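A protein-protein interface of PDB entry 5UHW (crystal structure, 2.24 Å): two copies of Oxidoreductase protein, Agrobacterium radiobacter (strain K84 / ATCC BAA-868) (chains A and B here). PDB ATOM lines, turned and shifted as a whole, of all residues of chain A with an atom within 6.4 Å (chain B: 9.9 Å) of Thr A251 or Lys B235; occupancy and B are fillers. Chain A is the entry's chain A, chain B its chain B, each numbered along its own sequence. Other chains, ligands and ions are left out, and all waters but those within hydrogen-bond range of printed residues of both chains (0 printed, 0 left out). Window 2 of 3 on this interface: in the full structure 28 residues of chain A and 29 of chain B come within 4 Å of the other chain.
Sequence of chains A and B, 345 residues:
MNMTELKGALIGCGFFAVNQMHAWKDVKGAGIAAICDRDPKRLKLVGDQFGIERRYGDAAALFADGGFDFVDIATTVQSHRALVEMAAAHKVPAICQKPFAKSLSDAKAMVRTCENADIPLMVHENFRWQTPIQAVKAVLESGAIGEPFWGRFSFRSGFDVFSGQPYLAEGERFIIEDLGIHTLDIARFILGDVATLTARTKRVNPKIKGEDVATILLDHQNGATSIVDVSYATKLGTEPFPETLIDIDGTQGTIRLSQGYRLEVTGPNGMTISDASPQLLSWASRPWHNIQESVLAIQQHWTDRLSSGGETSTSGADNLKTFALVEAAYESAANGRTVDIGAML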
ATOM      1  N   ILE A 145      10.680   7.616  28.921  1.00  0.00           N
ATOM      2  CA  ILE A 145      10.206   6.241  28.970  1.00  0.00           C
ATOM      3  C   ILE A 145       8.726   6.105  28.644  1.00  0.00           C
ATOM      4  O   ILE A 145       8.150   5.044  28.895  1.00  0.00           O
ATOM      5  CB  ILE A 145      10.486   5.610  30.352  1.00  0.00           C
ATOM      6  CG1 ILE A 145       9.731   6.332  31.483  1.00  0.00           C
ATOM      7  CG2 ILE A 145      11.984   5.580  30.643  1.00  0.00           C
ATOM      8  CD1 ILE A 145       9.525   5.431  32.694  1.00  0.00           C
ATOM      9  N   GLY A 146       8.115   7.146  28.077  1.00  0.00           N
ATOM     10  CA  GLY A 146       6.695   7.128  27.749  1.00  0.00           C
ATOM     11  C   GLY A 146       5.818   7.330  28.962  1.00  0.00           C
ATOM     12  O   GLY A 146       6.291   7.805  30.001  1.00  0.00           O
ATOM     13  N   GLU A 147       4.537   6.975  28.821  1.00  0.00           N
ATOM     14  CA  GLU A 147       3.572   6.999  29.935  1.00  0.00           C
ATOM     15  C   GLU A 147       3.938   5.910  30.964  1.00  0.00           C
ATOM     16  O   GLU A 147       4.066   4.740  30.591  1.00  0.00           O
ATOM     17  CB  GLU A 147       2.123   6.711  29.453  1.00  0.00           C
ATOM     18  CG  GLU A 147       1.498   7.650  28.403  1.00  0.00           C
ATOM     19  CD  GLU A 147       1.183   9.062  28.932  1.00  0.00           C
ATOM     20  OE1 GLU A 147       1.395   9.332  30.161  1.00  0.00           O
ATOM     21  OE2 GLU A 147       0.725   9.913  28.109  1.00  0.00           O
ATOM     22  N   PRO A 148       4.082   6.274  32.257  1.00  0.00           N
ATOM     23  CA  PRO A 148       4.318   5.211  33.249  1.00  0.00           C
ATOM     24  C   PRO A 148       3.048   4.375  33.473  1.00  0.00           C
ATOM     25  O   PRO A 148       1.961   4.938  33.483  1.00  0.00           O
ATOM     26  CB  PRO A 148       4.677   5.995  34.512  1.00  0.00           C
ATOM     27  CG  PRO A 148       3.923   7.276  34.371  1.00  0.00           C
ATOM     28  CD  PRO A 148       3.959   7.598  32.904  1.00  0.00           C
ATOM     29  N   PHE A 149       3.195   3.054  33.596  1.00  0.00           N
ATOM     30  CA  PHE A 149       2.077   2.143  33.936  1.00  0.00           C
ATOM     31  C   PHE A 149       2.286   1.264  35.193  1.00  0.00           C
ATOM     32  O   PHE A 149       1.323   0.676  35.696  1.00  0.00           O
ATOM     33  CB  PHE A 149       1.737   1.252  32.731  1.00  0.00           C
ATOM     34  CG  PHE A 149       2.815   0.264  32.353  1.00  0.00           C
ATOM     35  CD1 PHE A 149       2.952  -0.942  33.033  1.00  0.00           C
ATOM     36  CD2 PHE A 149       3.671   0.521  31.282  1.00  0.00           C
ATOM     37  CE1 PHE A 149       3.936  -1.850  32.676  1.00  0.00           C
ATOM     38  CE2 PHE A 149       4.651  -0.407  30.903  1.00  0.00           C
ATOM     39  CZ  PHE A 149       4.783  -1.590  31.604  1.00  0.00           C
ATOM     40  N   ASP A 249       8.081   1.297  35.201  1.00  0.00           N
ATOM     41  CA  ASP A 249       7.957   0.808  33.823  1.00  0.00           C
ATOM     42  C   ASP A 249       7.048   1.719  33.046  1.00  0.00           C
ATOM     43  O   ASP A 249       5.946   2.017  33.491  1.00  0.00           O
ATOM     44  CB  ASP A 249       7.416  -0.625  33.765  1.00  0.00           C
ATOM     45  CG  ASP A 249       8.410  -1.652  34.258  1.00  0.00           C
ATOM     46  OD1 ASP A 249       9.543  -1.267  34.642  1.00  0.00           O
ATOM     47  OD2 ASP A 249       8.066  -2.853  34.257  1.00  0.00           O
ATOM     48  N   GLY A 250       7.529   2.171  31.890  1.00  0.00           N
ATOM     49  CA  GLY A 250       6.750   2.989  30.974  1.00  0.00           C
ATOM     50  C   GLY A 250       6.592   2.328  29.624  1.00  0.00           C
ATOM     51  O   GLY A 250       7.275   1.355  29.315  1.00  0.00           O
ATOM     52  N   THR A 251       5.702   2.898  28.811  1.00  0.00           N
ATOM     53  CA  THR A 251       5.360   2.375  27.469  1.00  0.00           C
ATOM     54  C   THR A 251       6.531   2.358  26.469  1.00  0.00           C
ATOM     55  O   THR A 251       6.466   1.647  25.470  1.00  0.00           O
ATOM     56  CB  THR A 251       4.234   3.219  26.821  1.00  0.00           C
ATOM     57  OG1 THR A 251       4.664   4.584  26.726  1.00  0.00           O
ATOM     58  CG2 THR A 251       2.904   3.143  27.631  1.00  0.00           C
ATOM     59  N   GLN A 252       7.567   3.172  26.716  1.00  0.00           N
ATOM     60  CA  GLN A 252       8.781   3.224  25.879  1.00  0.00           C
ATOM     61  C   GLN A 252      10.094   3.029  26.648  1.00  0.00           C
ATOM     62  O   GLN A 252      11.166   3.294  26.111  1.00  0.00           O
ATOM     63  CB  GLN A 252       8.819   4.569  25.161  1.00  0.00           C
ATOM     64  CG  GLN A 252       7.845   4.677  24.006  1.00  0.00           C
ATOM     65  CD  GLN A 252       7.613   6.131  23.619  1.00  0.00           C
ATOM     66  OE1 GLN A 252       8.473   7.005  23.853  1.00  0.00           O
ATOM     67  NE2 GLN A 252       6.449   6.404  23.021  1.00  0.00           N
ATOM     68  N   GLY A 253      10.030   2.568  27.889  1.00  0.00           N
ATOM     69  CA  GLY A 253      11.248   2.408  28.664  1.00  0.00           C
ATOM     70  C   GLY A 253      11.059   2.074  30.120  1.00  0.00           C
ATOM     71  O   GLY A 253       9.979   1.737  30.549  1.00  0.00           O
ATOM     72  N   THR A 254      12.145   2.184  30.869  1.00  0.00           N
ATOM     73  CA  THR A 254      12.192   1.813  32.285  1.00  0.00           C
ATOM     74  C   THR A 254      13.157   2.713  33.068  1.00  0.00           C
ATOM     75  O   THR A 254      14.137   3.229  32.502  1.00  0.00           O
ATOM     76  CB  THR A 254      12.655   0.354  32.502  1.00  0.00           C
ATOM     77  OG1 THR A 254      13.967   0.161  31.964  1.00  0.00           O
ATOM     78  CG2 THR A 254      11.662  -0.673  31.882  1.00  0.00           C
ATOM     79  N   THR A 266      16.358   3.325  30.501  1.00  0.00           N
ATOM     80  CA  THR A 266      16.413   2.827  29.140  1.00  0.00           C
ATOM     81  C   THR A 266      15.204   3.316  28.371  1.00  0.00           C
ATOM     82  O   THR A 266      14.097   3.367  28.896  1.00  0.00           O
ATOM     83  CB  THR A 266      16.569   1.304  29.049  1.00  0.00           C
ATOM     84  OG1 THR A 266      15.363   0.690  29.465  1.00  0.00           O
ATOM     85  CG2 THR A 266      17.713   0.803  29.914  1.00  0.00           C
ATOM     86  N   GLY A 267      15.461   3.691  27.125  1.00  0.00           N
ATOM     87  CA  GLY A 267      14.479   4.319  26.262  1.00  0.00           C
ATOM     88  C   GLY A 267      14.671   3.815  24.856  1.00  0.00           C
ATOM     89  O   GLY A 267      15.449   2.914  24.633  1.00  0.00           O
ATOM     90  N   ARG B 156       9.742  -9.892  34.511  1.00  0.00           N
ATOM     91  CA  ARG B 156       9.507  -8.675  33.746  1.00  0.00           C
ATOM     92  C   ARG B 156      10.407  -8.727  32.509  1.00  0.00           C
ATOM     93  O   ARG B 156      11.630  -8.726  32.626  1.00  0.00           O
ATOM     94  CB  ARG B 156       9.820  -7.425  34.592  1.00  0.00           C
ATOM     95  CG  ARG B 156       9.057  -7.364  35.903  1.00  0.00           C
ATOM     96  CD  ARG B 156       9.018  -5.968  36.510  1.00  0.00           C
ATOM     97  NE  ARG B 156       8.005  -5.099  35.906  1.00  0.00           N
ATOM     98  CZ  ARG B 156       6.684  -5.183  36.100  1.00  0.00           C
ATOM     99  NH1 ARG B 156       6.144  -6.112  36.896  1.00  0.00           N
ATOM    100  NH2 ARG B 156       5.879  -4.333  35.480  1.00  0.00           N
ATOM    101  N   SER B 157       9.794  -8.764  31.339  1.00  0.00           N
ATOM    102  CA  SER B 157      10.498  -9.006  30.101  1.00  0.00           C
ATOM    103  C   SER B 157       9.973  -8.060  29.024  1.00  0.00           C
ATOM    104  O   SER B 157       8.860  -7.541  29.139  1.00  0.00           O
ATOM    105  CB  SER B 157      10.243 -10.453  29.701  1.00  0.00           C
ATOM    106  OG  SER B 157      11.082 -10.843  28.660  1.00  0.00           O
ATOM    107  N   GLY B 158      10.796  -7.814  28.007  1.00  0.00           N
ATOM    108  CA  GLY B 158      10.381  -7.137  26.768  1.00  0.00           C
ATOM    109  C   GLY B 158      10.583  -8.038  25.553  1.00  0.00           C
ATOM    110  O   GLY B 158      10.578  -7.574  24.418  1.00  0.00           O
ATOM    111  N   PHE B 159      10.735  -9.338  25.803  1.00  0.00           N
ATOM    112  CA  PHE B 159      11.092 -10.313  24.784  1.00  0.00           C
ATOM    113  C   PHE B 159       9.886 -10.542  23.910  1.00  0.00           C
ATOM    114  O   PHE B 159       8.788 -10.746  24.418  1.00  0.00           O
ATOM    115  CB  PHE B 159      11.502 -11.629  25.461  1.00  0.00           C
ATOM    116  CG  PHE B 159      12.062 -12.663  24.521  1.00  0.00           C
ATOM    117  CD1 PHE B 159      13.430 -12.685  24.215  1.00  0.00           C
ATOM    118  CD2 PHE B 159      11.231 -13.637  23.957  1.00  0.00           C
ATOM    119  CE1 PHE B 159      13.947 -13.645  23.354  1.00  0.00           C
ATOM    120  CE2 PHE B 159      11.741 -14.593  23.092  1.00  0.00           C
ATOM    121  CZ  PHE B 159      13.100 -14.601  22.793  1.00  0.00           C
ATOM    122  N   ASP B 160      10.100 -10.499  22.602  1.00  0.00           N
ATOM    123  CA  ASP B 160       9.064 -10.811  21.613  1.00  0.00           C
ATOM    124  C   ASP B 160       8.764 -12.337  21.609  1.00  0.00           C
ATOM    125  O   ASP B 160       9.304 -13.083  20.787  1.00  0.00           O
ATOM    126  CB  ASP B 160       9.528 -10.291  20.226  1.00  0.00           C
ATOM    127  CG  ASP B 160       8.438 -10.359  19.131  1.00  0.00           C
ATOM    128  OD1 ASP B 160       7.414 -11.059  19.296  1.00  0.00           O
ATOM    129  OD2 ASP B 160       8.633  -9.700  18.081  1.00  0.00           O
ATOM    130  N   PHE B 162       5.789 -13.318  20.896  1.00  0.00           N
ATOM    131  CA  PHE B 162       4.705 -13.365  19.917  1.00  0.00           C
ATOM    132  C   PHE B 162       5.151 -13.912  18.536  1.00  0.00           C
ATOM    133  O   PHE B 162       4.297 -14.286  17.728  1.00  0.00           O
ATOM    134  CB  PHE B 162       4.053 -11.971  19.772  1.00  0.00           C
ATOM    135  CG  PHE B 162       3.755 -11.284  21.095  1.00  0.00           C
ATOM    136  CD1 PHE B 162       2.942 -11.899  22.054  1.00  0.00           C
ATOM    137  CD2 PHE B 162       4.283 -10.015  21.381  1.00  0.00           C
ATOM    138  CE1 PHE B 162       2.668 -11.272  23.265  1.00  0.00           C
ATOM    139  CE2 PHE B 162       4.010  -9.389  22.593  1.00  0.00           C
ATOM    140  CZ  PHE B 162       3.203 -10.018  23.536  1.00  0.00           C
ATOM    141  N   LYS B 202      -3.434  -5.003  33.239  1.00  0.00           N
ATOM    142  CA  LYS B 202      -3.314  -3.871  32.333  1.00  0.00           C
ATOM    143  C   LYS B 202      -2.879  -4.420  30.982  1.00  0.00           C
ATOM    144  O   LYS B 202      -2.120  -5.395  30.927  1.00  0.00           O
ATOM    145  CB  LYS B 202      -2.263  -2.891  32.862  1.00  0.00           C
ATOM    146  CG  LYS B 202      -2.593  -1.423  32.682  1.00  0.00           C
ATOM    147  CD  LYS B 202      -1.741  -0.513  33.558  1.00  0.00           C
ATOM    148  CE  LYS B 202      -1.930  -0.782  35.058  1.00  0.00           C
ATOM    149  NZ  LYS B 202      -1.001  -1.829  35.629  1.00  0.00           N
ATOM    150  N   ARG B 203      -3.373  -3.820  29.905  1.00  0.00           N
ATOM    151  CA  ARG B 203      -2.872  -4.105  28.570  1.00  0.00           C
ATOM    152  C   ARG B 203      -2.089  -2.889  28.105  1.00  0.00           C
ATOM    153  O   ARG B 203      -2.647  -1.803  28.053  1.00  0.00           O
ATOM    154  CB  ARG B 203      -4.034  -4.388  27.623  1.00  0.00           C
ATOM    155  CG  ARG B 203      -3.665  -5.298  26.458  1.00  0.00           C
ATOM    156  CD  ARG B 203      -3.560  -4.591  25.118  1.00  0.00           C
ATOM    157  NE  ARG B 203      -4.843  -4.594  24.402  1.00  0.00           N
ATOM    158  CZ  ARG B 203      -5.521  -3.521  23.984  1.00  0.00           C
ATOM    159  NH1 ARG B 203      -5.089  -2.270  24.173  1.00  0.00           N
ATOM    160  NH2 ARG B 203      -6.672  -3.707  23.347  1.00  0.00           N
ATOM    161  N   VAL B 204      -0.790  -3.047  27.824  1.00  0.00           N
ATOM    162  CA  VAL B 204       0.056  -1.919  27.351  1.00  0.00           C
ATOM    163  C   VAL B 204       0.315  -2.005  25.837  1.00  0.00           C
ATOM    164  O   VAL B 204       0.219  -1.009  25.120  1.00  0.00           O
ATOM    165  CB  VAL B 204       1.411  -1.851  28.101  1.00  0.00           C
ATOM    166  CG1 VAL B 204       2.159  -0.567  27.762  1.00  0.00           C
ATOM    167  CG2 VAL B 204       1.193  -1.975  29.602  1.00  0.00           C
ATOM    168  N   ASN B 205       0.653  -3.202  25.377  1.00  0.00           N
ATOM    169  CA  ASN B 205       0.997  -3.441  23.993  1.00  0.00           C
ATOM    170  C   ASN B 205      -0.222  -3.175  23.086  1.00  0.00           C
ATOM    171  O   ASN B 205      -1.221  -3.887  23.177  1.00  0.00           O
ATOM    172  CB  ASN B 205       1.493  -4.883  23.869  1.00  0.00           C
ATOM    173  CG  ASN B 205       2.097  -5.193  22.517  1.00  0.00           C
ATOM    174  OD1 ASN B 205       1.940  -4.435  21.557  1.00  0.00           O
ATOM    175  ND2 ASN B 205       2.797  -6.323  22.438  1.00  0.00           N
ATOM    176  N   PRO B 206      -0.142  -2.156  22.201  1.00  0.00           N
ATOM    177  CA  PRO B 206      -1.289  -1.894  21.309  1.00  0.00           C
ATOM    178  C   PRO B 206      -1.706  -3.058  20.406  1.00  0.00           C
ATOM    179  O   PRO B 206      -2.836  -3.054  19.972  1.00  0.00           O
ATOM    180  CB  PRO B 206      -0.810  -0.718  20.448  1.00  0.00           C
ATOM    181  CG  PRO B 206       0.267  -0.066  21.242  1.00  0.00           C
ATOM    182  CD  PRO B 206       0.950  -1.185  21.970  1.00  0.00           C
ATOM    183  N   LYS B 207      -0.821  -4.039  20.176  1.00  0.00           N
ATOM    184  CA  LYS B 207      -1.003  -5.123  19.191  1.00  0.00           C
ATOM    185  C   LYS B 207      -1.463  -6.478  19.738  1.00  0.00           C
ATOM    186  O   LYS B 207      -1.269  -7.493  19.064  1.00  0.00           O
ATOM    187  CB  LYS B 207       0.320  -5.370  18.427  1.00  0.00           C
ATOM    188  CG  LYS B 207       1.067  -4.097  18.063  1.00  0.00           C
ATOM    189  CD  LYS B 207       2.036  -4.275  16.911  1.00  0.00           C
ATOM    190  CE  LYS B 207       2.490  -2.907  16.437  1.00  0.00           C
ATOM    191  NZ  LYS B 207       3.365  -2.996  15.249  1.00  0.00           N
ATOM    192  N   ASP B 212      -1.050  -7.829  29.443  1.00  0.00           N
ATOM    193  CA  ASP B 212       0.373  -8.187  29.443  1.00  0.00           C
ATOM    194  C   ASP B 212       1.153  -7.731  30.676  1.00  0.00           C
ATOM    195  O   ASP B 212       2.373  -7.947  30.750  1.00  0.00           O
ATOM    196  CB  ASP B 212       1.059  -7.760  28.134  1.00  0.00           C
ATOM    197  CG  ASP B 212       0.956  -6.289  27.855  1.00  0.00           C
ATOM    198  OD1 ASP B 212       0.242  -5.567  28.579  1.00  0.00           O
ATOM    199  OD2 ASP B 212       1.592  -5.842  26.876  1.00  0.00           O
ATOM    200  N   VAL B 213       0.449  -7.121  31.633  1.00  0.00           N
ATOM    201  CA  VAL B 213       1.014  -6.751  32.919  1.00  0.00           C
ATOM    202  C   VAL B 213       0.039  -7.230  33.967  1.00  0.00           C
ATOM    203  O   VAL B 213      -1.173  -7.033  33.819  1.00  0.00           O
ATOM    204  CB  VAL B 213       1.198  -5.235  33.039  1.00  0.00           C
ATOM    205  CG1 VAL B 213       1.853  -4.860  34.374  1.00  0.00           C
ATOM    206  CG2 VAL B 213       2.017  -4.715  31.858  1.00  0.00           C
ATOM    207  N   SER B 231       5.281  -9.141  33.675  1.00  0.00           N
ATOM    208  CA  SER B 231       5.137  -8.164  32.584  1.00  0.00           C
ATOM    209  C   SER B 231       5.856  -8.631  31.330  1.00  0.00           C
ATOM    210  O   SER B 231       6.983  -9.128  31.417  1.00  0.00           O
ATOM    211  CB  SER B 231       5.726  -6.815  32.979  1.00  0.00           C
ATOM    212  OG  SER B 231       5.749  -5.885  31.880  1.00  0.00           O
ATOM    213  N   TYR B 232       5.196  -8.470  30.171  1.00  0.00           N
ATOM    214  CA  TYR B 232       5.853  -8.561  28.850  1.00  0.00           C
ATOM    215  C   TYR B 232       5.907  -7.209  28.147  1.00  0.00           C
ATOM    216  O   TYR B 232       6.152  -7.163  26.951  1.00  0.00           O
ATOM    217  CB  TYR B 232       5.179  -9.614  27.962  1.00  0.00           C
ATOM    218  CG  TYR B 232       5.764 -10.999  28.115  1.00  0.00           C
ATOM    219  CD1 TYR B 232       7.091 -11.253  27.779  1.00  0.00           C
ATOM    220  CD2 TYR B 232       4.980 -12.078  28.566  1.00  0.00           C
ATOM    221  CE1 TYR B 232       7.627 -12.522  27.903  1.00  0.00           C
ATOM    222  CE2 TYR B 232       5.513 -13.362  28.689  1.00  0.00           C
ATOM    223  CZ  TYR B 232       6.839 -13.568  28.358  1.00  0.00           C
ATOM    224  OH  TYR B 232       7.391 -14.805  28.473  1.00  0.00           O
ATOM    225  N   ALA B 233       5.742  -6.117  28.891  1.00  0.00           N
ATOM    226  CA  ALA B 233       5.856  -4.767  28.348  1.00  0.00           C
ATOM    227  C   ALA B 233       6.957  -3.970  29.036  1.00  0.00           C
ATOM    228  O   ALA B 233       6.870  -2.752  29.141  1.00  0.00           O
ATOM    229  CB  ALA B 233       4.525  -4.059  28.491  1.00  0.00           C
ATOM    230  N   THR B 234       8.002  -4.655  29.495  1.00  0.00           N
ATOM    231  CA  THR B 234       9.066  -4.039  30.300  1.00  0.00           C
ATOM    232  C   THR B 234      10.337  -4.030  29.460  1.00  0.00           C
ATOM    233  O   THR B 234      10.856  -5.075  29.108  1.00  0.00           O
ATOM    234  CB  THR B 234       9.278  -4.809  31.639  1.00  0.00           C
ATOM    235  OG1 THR B 234       8.064  -4.804  32.394  1.00  0.00           O
ATOM    236  CG2 THR B 234      10.366  -4.181  32.489  1.00  0.00           C
ATOM    237  N   LYS B 235      10.835  -2.845  29.153  1.00  0.00           N
ATOM    238  CA  LYS B 235      11.939  -2.682  28.232  1.00  0.00           C
ATOM    239  C   LYS B 235      13.197  -2.287  28.974  1.00  0.00           C
ATOM    240  O   LYS B 235      13.396  -1.120  29.279  1.00  0.00           O
ATOM    241  CB  LYS B 235      11.562  -1.629  27.204  1.00  0.00           C
ATOM    242  CG  LYS B 235      10.337  -2.024  26.381  1.00  0.00           C
ATOM    243  CD  LYS B 235       9.917  -0.878  25.461  1.00  0.00           C
ATOM    244  CE  LYS B 235       9.111  -1.332  24.248  1.00  0.00           C
ATOM    245  NZ  LYS B 235       7.652  -1.189  24.476  1.00  0.00           N
ATOM    246  N   LEU B 236      14.043  -3.270  29.263  1.00  0.00           N
ATOM    247  CA  LEU B 236      15.283  -3.057  30.022  1.00  0.00           C
ATOM    248  C   LEU B 236      16.530  -3.064  29.124  1.00  0.00           C
ATOM    249  O   LEU B 236      16.489  -3.537  27.985  1.00  0.00           O
ATOM    250  CB  LEU B 236      15.422  -4.157  31.075  1.00  0.00           C
ATOM    251  CG  LEU B 236      14.389  -4.210  32.213  1.00  0.00           C
ATOM    252  CD1 LEU B 236      14.250  -5.637  32.743  1.00  0.00           C
ATOM    253  CD2 LEU B 236      14.756  -3.227  33.332  1.00  0.00           C
ATOM    254  N   GLY B 237      17.643  -2.575  29.674  1.00  0.00           N
ATOM    255  CA  GLY B 237      18.940  -2.503  28.960  1.00  0.00           C
ATOM    256  C   GLY B 237      19.752  -3.790  28.837  1.00  0.00           C
ATOM    257  O   GLY B 237      20.696  -3.859  28.050  1.00  0.00           O
ATOM    258  N   THR B 238      19.425  -4.783  29.654  1.00  0.00           N
ATOM    259  CA  THR B 238      19.855  -6.171  29.450  1.00  0.00           C
ATOM    260  C   THR B 238      18.579  -7.017  29.654  1.00  0.00           C
ATOM    261  O   THR B 238      17.879  -6.869  30.652  1.00  0.00           O
ATOM    262  CB  THR B 238      21.015  -6.574  30.405  1.00  0.00           C
ATOM    263  OG1 THR B 238      20.729  -6.101  31.712  1.00  0.00           O
ATOM    264  CG2 THR B 238      22.364  -5.928  30.000  1.00  0.00           C
ATOM    265  N   GLU B 239      18.254  -7.849  28.670  1.00  0.00           N
ATOM    266  CA  GLU B 239      16.997  -8.598  28.662  1.00  0.00           C
ATOM    267  C   GLU B 239      17.065  -9.805  29.630  1.00  0.00           C
ATOM    268  O   GLU B 239      17.884 -10.687  29.416  1.00  0.00           O
ATOM    269  CB  GLU B 239      16.684  -9.058  27.212  1.00  0.00           C
ATOM    270  CG  GLU B 239      15.447  -9.929  27.053  1.00  0.00           C
ATOM    271  CD  GLU B 239      14.229  -9.343  27.752  1.00  0.00           C
ATOM    272  OE1 GLU B 239      13.892  -8.171  27.460  1.00  0.00           O
ATOM    273  OE2 GLU B 239      13.626 -10.035  28.607  1.00  0.00           O
ATOM    274  N   PRO B 240      16.204  -9.857  30.686  1.00  0.00           N
ATOM    275  CA  PRO B 240      16.276 -11.021  31.614  1.00  0.00           C
ATOM    276  C   PRO B 240      15.524 -12.302  31.195  1.00  0.00           C
ATOM    277  O   PRO B 240      15.553 -13.275  31.934  1.00  0.00           O
ATOM    278  CB  PRO B 240      15.658 -10.453  32.920  1.00  0.00           C
ATOM    279  CG  PRO B 240      14.617  -9.526  32.409  1.00  0.00           C
ATOM    280  CD  PRO B 240      15.236  -8.855  31.194  1.00  0.00           C
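O of Thr A251 sits at hydrogen-bond distance from NZ of Lys B235 (3.2 Å).
O of Phe A149 lies within hydrogen-bond range of NZ of Lys B202 (3.4 Å).
OG1 of Thr A266 sits at hydrogen-bond distance from O of Lys B235 (2.7 Å).
The side-chain carboxylate (OD2) of Asp A249 lies within salt-bridge range of the guanidinium group (NE) of Arg B156 (2.8 Å).
OD2 of Asp A249 is in hydrogen-bond range of OG1 of Thr B234, 2.7 Å away.
OG1 of Thr A254 lies within hydrogen-bond range of O of Lys B235.
The side-chain hydroxyl (OG1) of Thr A266 is in hydrogen-bond range of the side-chain hydroxyl (OG1) of Thr A254 (2.9 Å).
The backbone NH (N) of Gly B158 sits at hydrogen-bond distance from the backbone carbonyl oxygen (O) of Thr B234 (3.0 Å).
O of Lys B202 sits at hydrogen-bond distance from N of Asp B212 (3.0 Å).
N of Ala B233 lies within hydrogen-bond range of O of Ser B157 (3.4 Å).
The backbone NH of Thr B234 is in hydrogen-bond range of the backbone carbonyl oxygen of Ser B157 (3.0 Å).
O of Ile A145 lies within hydrogen-bond range of N of Thr A251, 3.3 Å away.
Phe A149 touches Val B204.
Val B213 touches Phe A149 (CG2 to CE1, 3.5 Å).
CZ of Phe A149 touches O of Ala B233, 3.4 Å away.
Val B204 touches Thr A251 (CG1 to CG2, 3.8 Å).
Thr B234 touches Thr A254.
CD2 of Leu B236 touches OG1 of Thr A254 (3.7 Å).
CA of Leu B236 touches OG1 of Thr A266, at 3.8 Å.
Thr A266 touches Gly B237.
No residue of chain B comes within 4 Å of Gly A146.
Printed residues of chain B within 4 Å of Phe A149: Lys B202, Val B204, Val B213 and Ala B233.
No residue of chain B comes within 4 Å of Gly A250.
Thr A251 touches two residues of chain B.
No residue of chain B comes within 4 Å of Gln A252.
Of the printed residues of chain B, Thr A266 touches Lys B235 (2.7 Å), Leu B236 (3.8 Å) and Gly B237 (3.4 Å).
Phe B159 touches none of the printed residues of chain A.
Printed residues of chain A within 4 Å of Val B204: Phe A149 and Thr A251.
Printed residues of chain A within 4 Å of Val B213: Phe A149.
Of the printed residues of chain A, Ala B233 touches Phe A149 (3.4 Å).
Lys B235 touches three residues of chain A.
Of the printed residues of chain A, Leu B236 touches Thr A254 (3.7 Å) and Thr A266 (3.8 Å).
The nearest residue of chain B that does not touch Thr A251 is Ala B233 (5.6 Å).
The nearest printed residue of chain A that does not touch Thr B234 is Phe A149 (4.7 Å).
Of the 24 printed residues of chain B, 9 touch a printed residue of chain A.
Hydrophobic or aromatic side chains of chain B within 4 Å of the printed part of chain A: Val B204, Val B213, Ala B233 and Leu B236.
Along chain B the printed residues that touch a printed residue of chain A span positions 156 to 237.
Hydrophobic or aromatic side chains of chain A that line the printed part of chain B: Phe A149.
No position is printed for both chains.
Of the 14 pairs that touch across the chains among the printed residues, none has its exchanged pair printed and touching as well.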
